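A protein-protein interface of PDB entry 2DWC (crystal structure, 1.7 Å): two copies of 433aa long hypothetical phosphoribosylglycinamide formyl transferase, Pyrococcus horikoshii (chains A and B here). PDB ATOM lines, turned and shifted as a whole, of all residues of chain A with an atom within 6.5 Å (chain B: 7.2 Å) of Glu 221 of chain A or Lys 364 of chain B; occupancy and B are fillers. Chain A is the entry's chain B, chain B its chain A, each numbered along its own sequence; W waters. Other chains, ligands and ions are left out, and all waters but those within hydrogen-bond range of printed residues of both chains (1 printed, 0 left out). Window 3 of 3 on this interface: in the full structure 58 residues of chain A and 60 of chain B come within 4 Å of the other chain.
OG of Ser 367 of chain B lies within hydrogen-bond range of O of Val 363 of chain B, at 2.7 Å.
Of the 12 printed residues of chain B, 6 touch a printed residue of chain A. Hydrophobic or aromatic side chains of chain B that line the printed part of chain A: Leu 362, Val 363 and Leu 366. Of the 10 printed residues of chain A, 4 touch a printed residue of chain B. Hydrophobic or aromatic side chains of chain A that line the printed part of chain B: Leu 7 and Pro 325.
Among the printed residues, pairs that only touch across the chains: Glu 221 of chain A with Val 363 of chain B (3.4 Å), Pro 325 of chain A with Ser 367 of chain B (3.5 Å), Glu 221 of chain A with Ser 367 of chain B (3.6 Å), Glu 221 of chain A with Lys 364 of chain B (3.7 Å), Leu 7 of chain A with Val 363 of chain B (3.7 Å), Pro 325 of chain A with Val 363 of chain B (3.7 Å), Pro 325 of chain A with Leu 366 of chain B (3.8 Å) and Pro 325 of chain A with Leu 362 of chain B (3.9 Å).
Glu 221 of chain A touches just these residues of chain B: Val 363, Lys 364 and Ser 367. Of the printed residues of chain A, Lys 364 of chain B touches Glu 221 (3.7 Å). Of the printed residues of chain A, Gly 361 of chain B touches Asp 9. Of the printed residues of chain B, Asp 9 of chain A touches Gly 361, Leu 362 and Val 363. Printed residues of chain B within 4 Å of Pro 325 of chain A: Leu 362 (3.9 Å), Val 363 (3.7 Å), Leu 366 (3.8 Å) and Ser 367 (3.5 Å).
No position is printed for both chains. Of the 11 pairs that touch across the chains among the printed residues, none has its exchanged pair printed and touching as well.
N of Gly 361 of chain B sits at hydrogen-bond distance from OD2 of Asp 9 of chain A, 3.1 Å away. The side-chain carboxylate (OD1) of Asp 9 of chain A is in hydrogen-bond range of the backbone NH (N) of Leu 362 of chain B (3.0 Å). The backbone NH (N) of Val 363 of chain B is in hydrogen-bond range of the side-chain carboxylate (OD1) of Asp 9 of chain A, at 2.9 Å.
Water W1 lies within hydrogen-bond range of the side-chain carboxylate (OD1) of Asp 9 of chain A, the backbone NH (N) of Lys 364 of chain B and the backbone carbonyl oxygen (O) of Gly 361 of chain B.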
ATOM      1  N   LEU A   7     -10.883  -3.633   2.745  1.00  0.00           N
ATOM      2  CA  LEU A   7      -9.746  -4.464   2.320  1.00  0.00           C
ATOM      3  C   LEU A   7      -9.744  -5.730   3.183  1.00  0.00           C
ATOM      4  O   LEU A   7      -9.864  -5.688   4.443  1.00  0.00           O
ATOM      5  CB  LEU A   7      -8.432  -3.647   2.515  1.00  0.00           C
ATOM      6  CG  LEU A   7      -7.104  -4.395   2.278  1.00  0.00           C
ATOM      7  CD1 LEU A   7      -6.858  -4.655   0.822  1.00  0.00           C
ATOM      8  CD2 LEU A   7      -5.957  -3.529   2.824  1.00  0.00           C
ATOM      9  N   ASP A   9      -7.991  -9.333   4.437  1.00  0.00           N
ATOM     10  CA  ASP A   9      -6.716  -9.996   4.696  1.00  0.00           C
ATOM     11  C   ASP A   9      -6.926 -11.463   5.022  1.00  0.00           C
ATOM     12  O   ASP A   9      -5.958 -12.192   5.203  1.00  0.00           O
ATOM     13  CB  ASP A   9      -6.060  -9.335   5.924  1.00  0.00           C
ATOM     14  CG  ASP A   9      -4.662  -9.859   6.210  1.00  0.00           C
ATOM     15  OD1 ASP A   9      -3.801  -9.752   5.317  1.00  0.00           O
ATOM     16  OD2 ASP A   9      -4.433 -10.361   7.334  1.00  0.00           O
ATOM     17  N   PHE A 219      -9.253  -2.670  -4.003  1.00  0.00           N
ATOM     18  CA  PHE A 219      -8.443  -2.078  -2.936  1.00  0.00           C
ATOM     19  C   PHE A 219      -6.971  -2.308  -3.199  1.00  0.00           C
ATOM     20  O   PHE A 219      -6.563  -3.360  -3.724  1.00  0.00           O
ATOM     21  CB  PHE A 219      -8.743  -2.733  -1.582  1.00  0.00           C
ATOM     22  CG  PHE A 219     -10.072  -2.323  -0.987  1.00  0.00           C
ATOM     23  CD1 PHE A 219     -10.328  -0.981  -0.659  1.00  0.00           C
ATOM     24  CD2 PHE A 219     -11.094  -3.266  -0.821  1.00  0.00           C
ATOM     25  CE1 PHE A 219     -11.582  -0.581  -0.185  1.00  0.00           C
ATOM     26  CE2 PHE A 219     -12.357  -2.875  -0.349  1.00  0.00           C
ATOM     27  CZ  PHE A 219     -12.599  -1.515  -0.030  1.00  0.00           C
ATOM     28  N   ASP A 220      -6.168  -1.310  -2.851  1.00  0.00           N
ATOM     29  CA  ASP A 220      -4.723  -1.460  -2.938  1.00  0.00           C
ATOM     30  C   ASP A 220      -4.275  -1.890  -1.559  1.00  0.00           C
ATOM     31  O   ASP A 220      -5.073  -2.000  -0.614  1.00  0.00           O
ATOM     32  CB  ASP A 220      -4.021  -0.148  -3.379  1.00  0.00           C
ATOM     33  CG  ASP A 220      -4.201   1.023  -2.388  1.00  0.00           C
ATOM     34  OD1 ASP A 220      -4.537   0.826  -1.195  1.00  0.00           O
ATOM     35  OD2 ASP A 220      -3.965   2.176  -2.819  1.00  0.00           O
ATOM     36  N   GLU A 221      -2.975  -2.149  -1.416  1.00  0.00           N
ATOM     37  CA  GLU A 221      -2.467  -2.622  -0.151  1.00  0.00           C
ATOM     38  C   GLU A 221      -2.694  -1.680   1.021  1.00  0.00           C
ATOM     39  O   GLU A 221      -2.712  -2.114   2.173  1.00  0.00           O
ATOM     40  CB  GLU A 221      -0.969  -2.950  -0.302  1.00  0.00           C
ATOM     41  CG  GLU A 221      -0.501  -4.059   0.578  1.00  0.00           C
ATOM     42  CD  GLU A 221       0.952  -4.460   0.306  1.00  0.00           C
ATOM     43  OE1 GLU A 221       1.503  -4.076  -0.752  1.00  0.00           O
ATOM     44  OE2 GLU A 221       1.534  -5.169   1.153  1.00  0.00           O
ATOM     45  N   ASN A 222      -2.868  -0.392   0.734  1.00  0.00           N
ATOM     46  CA  ASN A 222      -3.110   0.595   1.783  1.00  0.00           C
ATOM     47  C   ASN A 222      -4.568   0.710   2.178  1.00  0.00           C
ATOM     48  O   ASN A 222      -4.910   1.475   3.070  1.00  0.00           O
ATOM     49  CB  ASN A 222      -2.629   1.984   1.360  1.00  0.00           C
ATOM     50  CG  ASN A 222      -1.177   1.993   0.989  1.00  0.00           C
ATOM     51  OD1 ASN A 222      -0.337   1.449   1.718  1.00  0.00           O
ATOM     52  ND2 ASN A 222      -0.856   2.614  -0.149  1.00  0.00           N
ATOM     53  N   GLY A 223      -5.443  -0.026   1.512  1.00  0.00           N
ATOM     54  CA  GLY A 223      -6.836   0.069   1.897  1.00  0.00           C
ATOM     55  C   GLY A 223      -7.639   1.076   1.106  1.00  0.00           C
ATOM     56  O   GLY A 223      -8.793   1.285   1.411  1.00  0.00           O
ATOM     57  N   GLU A 224      -7.033   1.729   0.119  1.00  0.00           N
ATOM     58  CA  GLU A 224      -7.790   2.682  -0.706  1.00  0.00           C
ATOM     59  C   GLU A 224      -8.159   2.037  -2.021  1.00  0.00           C
ATOM     60  O   GLU A 224      -7.532   1.088  -2.448  1.00  0.00           O
ATOM     61  CB  GLU A 224      -6.962   3.921  -0.985  1.00  0.00           C
ATOM     62  CG  GLU A 224      -6.621   4.591   0.306  1.00  0.00           C
ATOM     63  CD  GLU A 224      -5.740   5.787   0.118  1.00  0.00           C
ATOM     64  OE1 GLU A 224      -5.001   5.838  -0.900  1.00  0.00           O
ATOM     65  OE2 GLU A 224      -5.792   6.662   1.010  1.00  0.00           O
ATOM     66  N   PRO A 325      -6.524  -7.754  -2.775  1.00  0.00           N
ATOM     67  CA  PRO A 325      -5.694  -6.921  -3.638  1.00  0.00           C
ATOM     68  C   PRO A 325      -5.446  -7.594  -4.997  1.00  0.00           C
ATOM     69  O   PRO A 325      -5.676  -8.809  -5.190  1.00  0.00           O
ATOM     70  CB  PRO A 325      -4.392  -6.774  -2.833  1.00  0.00           C
ATOM     71  CG  PRO A 325      -4.329  -8.014  -2.041  1.00  0.00           C
ATOM     72  CD  PRO A 325      -5.760  -8.300  -1.640  1.00  0.00           C
ATOM     73  N   ARG A 335      -1.928   2.441 -13.571  1.00  0.00           N
ATOM     74  CA  ARG A 335      -1.637   1.174 -12.920  1.00  0.00           C
ATOM     75  C   ARG A 335      -2.147   0.136 -13.941  1.00  0.00           C
ATOM     76  O   ARG A 335      -3.353   0.027 -14.195  1.00  0.00           O
ATOM     77  CB  ARG A 335      -2.404   1.055 -11.594  1.00  0.00           C
ATOM     78  CG  ARG A 335      -1.809   0.041 -10.608  1.00  0.00           C
ATOM     79  CD  ARG A 335      -2.664  -0.053  -9.332  1.00  0.00           C
ATOM     80  NE  ARG A 335      -2.142  -0.919  -8.251  1.00  0.00           N
ATOM     81  CZ  ARG A 335      -2.308  -2.244  -8.165  1.00  0.00           C
ATOM     82  NH1 ARG A 335      -2.991  -2.912  -9.122  1.00  0.00           N
ATOM     83  NH2 ARG A 335      -1.831  -2.897  -7.093  1.00  0.00           N
ATOM     84  N   GLY B 361      -3.115 -12.898   6.257  1.00  0.00           N
ATOM     85  CA  GLY B 361      -1.866 -12.441   5.681  1.00  0.00           C
ATOM     86  C   GLY B 361      -2.062 -12.216   4.199  1.00  0.00           C
ATOM     87  O   GLY B 361      -1.104 -11.967   3.469  1.00  0.00           O
ATOM     88  N   LEU B 362      -3.323 -12.242   3.736  1.00  0.00           N
ATOM     89  CA  LEU B 362      -3.570 -12.107   2.309  1.00  0.00           C
ATOM     90  C   LEU B 362      -3.296 -10.727   1.711  1.00  0.00           C
ATOM     91  O   LEU B 362      -2.998 -10.643   0.517  1.00  0.00           O
ATOM     92  CB  LEU B 362      -5.017 -12.563   1.968  1.00  0.00           C
ATOM     93  CG  LEU B 362      -5.344 -13.987   2.409  1.00  0.00           C
ATOM     94  CD1 LEU B 362      -6.855 -14.323   2.041  1.00  0.00           C
ATOM     95  CD2 LEU B 362      -4.444 -14.990   1.698  1.00  0.00           C
ATOM     96  N   VAL B 363      -3.402  -9.642   2.488  1.00  0.00           N
ATOM     97  CA  VAL B 363      -3.097  -8.335   1.877  1.00  0.00           C
ATOM     98  C   VAL B 363      -1.660  -8.346   1.370  1.00  0.00           C
ATOM     99  O   VAL B 363      -1.376  -7.948   0.229  1.00  0.00           O
ATOM    100  CB  VAL B 363      -3.251  -7.172   2.896  1.00  0.00           C
ATOM    101  CG1 VAL B 363      -2.823  -5.818   2.273  1.00  0.00           C
ATOM    102  CG2 VAL B 363      -4.733  -7.038   3.252  1.00  0.00           C
ATOM    103  N   LYS B 364      -0.741  -8.801   2.215  1.00  0.00           N
ATOM    104  CA  LYS B 364       0.656  -8.835   1.746  1.00  0.00           C
ATOM    105  C   LYS B 364       0.887  -9.955   0.727  1.00  0.00           C
ATOM    106  O   LYS B 364       1.510  -9.738  -0.333  1.00  0.00           O
ATOM    107  CB  LYS B 364       1.607  -9.024   2.930  1.00  0.00           C
ATOM    108  CG  LYS B 364       1.742  -7.755   3.765  1.00  0.00           C
ATOM    109  CD  LYS B 364       2.732  -7.943   4.899  1.00  0.00           C
ATOM    110  CE  LYS B 364       2.821  -6.692   5.764  1.00  0.00           C
ATOM    111  NZ  LYS B 364       3.772  -6.883   6.917  1.00  0.00           N
ATOM    112  N   ALA B 365       0.386 -11.145   1.042  1.00  0.00           N
ATOM    113  CA  ALA B 365       0.608 -12.303   0.177  1.00  0.00           C
ATOM    114  C   ALA B 365       0.079 -12.116  -1.223  1.00  0.00           C
ATOM    115  O   ALA B 365       0.773 -12.445  -2.205  1.00  0.00           O
ATOM    116  CB  ALA B 365       0.006 -13.576   0.802  1.00  0.00           C
ATOM    117  N   LEU B 366      -1.140 -11.571  -1.339  1.00  0.00           N
ATOM    118  CA  LEU B 366      -1.741 -11.411  -2.651  1.00  0.00           C
ATOM    119  C   LEU B 366      -1.384 -10.126  -3.364  1.00  0.00           C
ATOM    120  O   LEU B 366      -1.911  -9.812  -4.436  1.00  0.00           O
ATOM    121  CB  LEU B 366      -3.282 -11.620  -2.576  1.00  0.00           C
ATOM    122  CG  LEU B 366      -3.642 -13.022  -2.065  1.00  0.00           C
ATOM    123  CD1 LEU B 366      -5.156 -13.120  -2.169  1.00  0.00           C
ATOM    124  CD2 LEU B 366      -2.966 -14.167  -2.867  1.00  0.00           C
ATOM    125  N   SER B 367      -0.479  -9.355  -2.766  1.00  0.00           N
ATOM    126  CA  SER B 367      -0.021  -8.150  -3.446  1.00  0.00           C
ATOM    127  C   SER B 367       1.285  -8.409  -4.203  1.00  0.00           C
ATOM    128  O   SER B 367       1.768  -7.522  -4.935  1.00  0.00           O
ATOM    129  CB  SER B 367       0.238  -7.017  -2.448  1.00  0.00           C
ATOM    130  OG  SER B 367      -0.992  -6.489  -1.986  1.00  0.00           O
ATOM    131  N   VAL B 368       1.857  -9.585  -4.005  1.00  0.00           N
ATOM    132  CA  VAL B 368       3.103  -9.946  -4.692  1.00  0.00           C
ATOM    133  C   VAL B 368       2.807 -10.180  -6.172  1.00  0.00           C
ATOM    134  O   VAL B 368       1.981 -11.031  -6.524  1.00  0.00           O
ATOM    135  CB  VAL B 368       3.686 -11.212  -4.090  1.00  0.00           C
ATOM    136  CG1 VAL B 368       4.931 -11.646  -4.884  1.00  0.00           C
ATOM    137  CG2 VAL B 368       3.993 -11.000  -2.607  1.00  0.00           C
ATOM    138  N   PRO B 369       3.487  -9.460  -7.078  1.00  0.00           N
ATOM    139  CA  PRO B 369       3.243  -9.640  -8.519  1.00  0.00           C
ATOM    140  C   PRO B 369       3.664 -11.037  -9.022  1.00  0.00           C
ATOM    141  O   PRO B 369       4.543 -11.677  -8.442  1.00  0.00           O
ATOM    142  CB  PRO B 369       4.104  -8.537  -9.176  1.00  0.00           C
ATOM    143  CG  PRO B 369       4.315  -7.559  -8.087  1.00  0.00           C
ATOM    144  CD  PRO B 369       4.471  -8.387  -6.849  1.00  0.00           C
ATOM    145  N   MET B 406       8.144 -17.120  -0.652  1.00  0.00           N
ATOM    146  CA  MET B 406       7.835 -15.880   0.051  1.00  0.00           C
ATOM    147  C   MET B 406       6.328 -15.721   0.289  1.00  0.00           C
ATOM    148  O   MET B 406       5.895 -15.405   1.391  1.00  0.00           O
ATOM    149  CB  MET B 406       8.338 -14.664  -0.733  1.00  0.00           C
ATOM    150  CG  MET B 406       8.024 -13.365  -0.028  1.00  0.00           C
ATOM    151  SD  MET B 406       8.712 -11.910  -0.842  1.00  0.00           S
ATOM    152  CE  MET B 406       7.318 -11.290  -1.748  1.00  0.00           C
ATOM    153  N   VAL B 407       5.541 -15.929  -0.758  1.00  0.00           N
ATOM    154  CA  VAL B 407       4.081 -15.806  -0.637  1.00  0.00           C
ATOM    155  C   VAL B 407       3.530 -16.826   0.351  1.00  0.00           C
ATOM    156  O   VAL B 407       2.677 -16.506   1.212  1.00  0.00           O
ATOM    157  CB  VAL B 407       3.430 -15.975  -2.045  1.00  0.00           C
ATOM    158  CG1 VAL B 407       1.925 -16.149  -1.896  1.00  0.00           C
ATOM    159  CG2 VAL B 407       3.736 -14.717  -2.901  1.00  0.00           C
ATOM    160  N   MET B 410       4.007 -15.800   3.946  1.00  0.00           N
ATOM    161  CA  MET B 410       3.237 -14.648   4.410  1.00  0.00           C
ATOM    162  C   MET B 410       1.857 -15.067   4.955  1.00  0.00           C
ATOM    163  O   MET B 410       1.115 -14.258   5.530  1.00  0.00           O
ATOM    164  CB  MET B 410       3.017 -13.667   3.267  1.00  0.00           C
ATOM    165  CG  MET B 410       4.268 -12.924   2.906  1.00  0.00           C
ATOM    166  SD  MET B 410       4.027 -11.977   1.412  1.00  0.00           S
ATOM    167  CE  MET B 410       4.463 -10.357   1.964  1.00  0.00           C
HETATM  168  O   HOH W   1      -1.204  -9.061   5.264  1.00  0.00           O
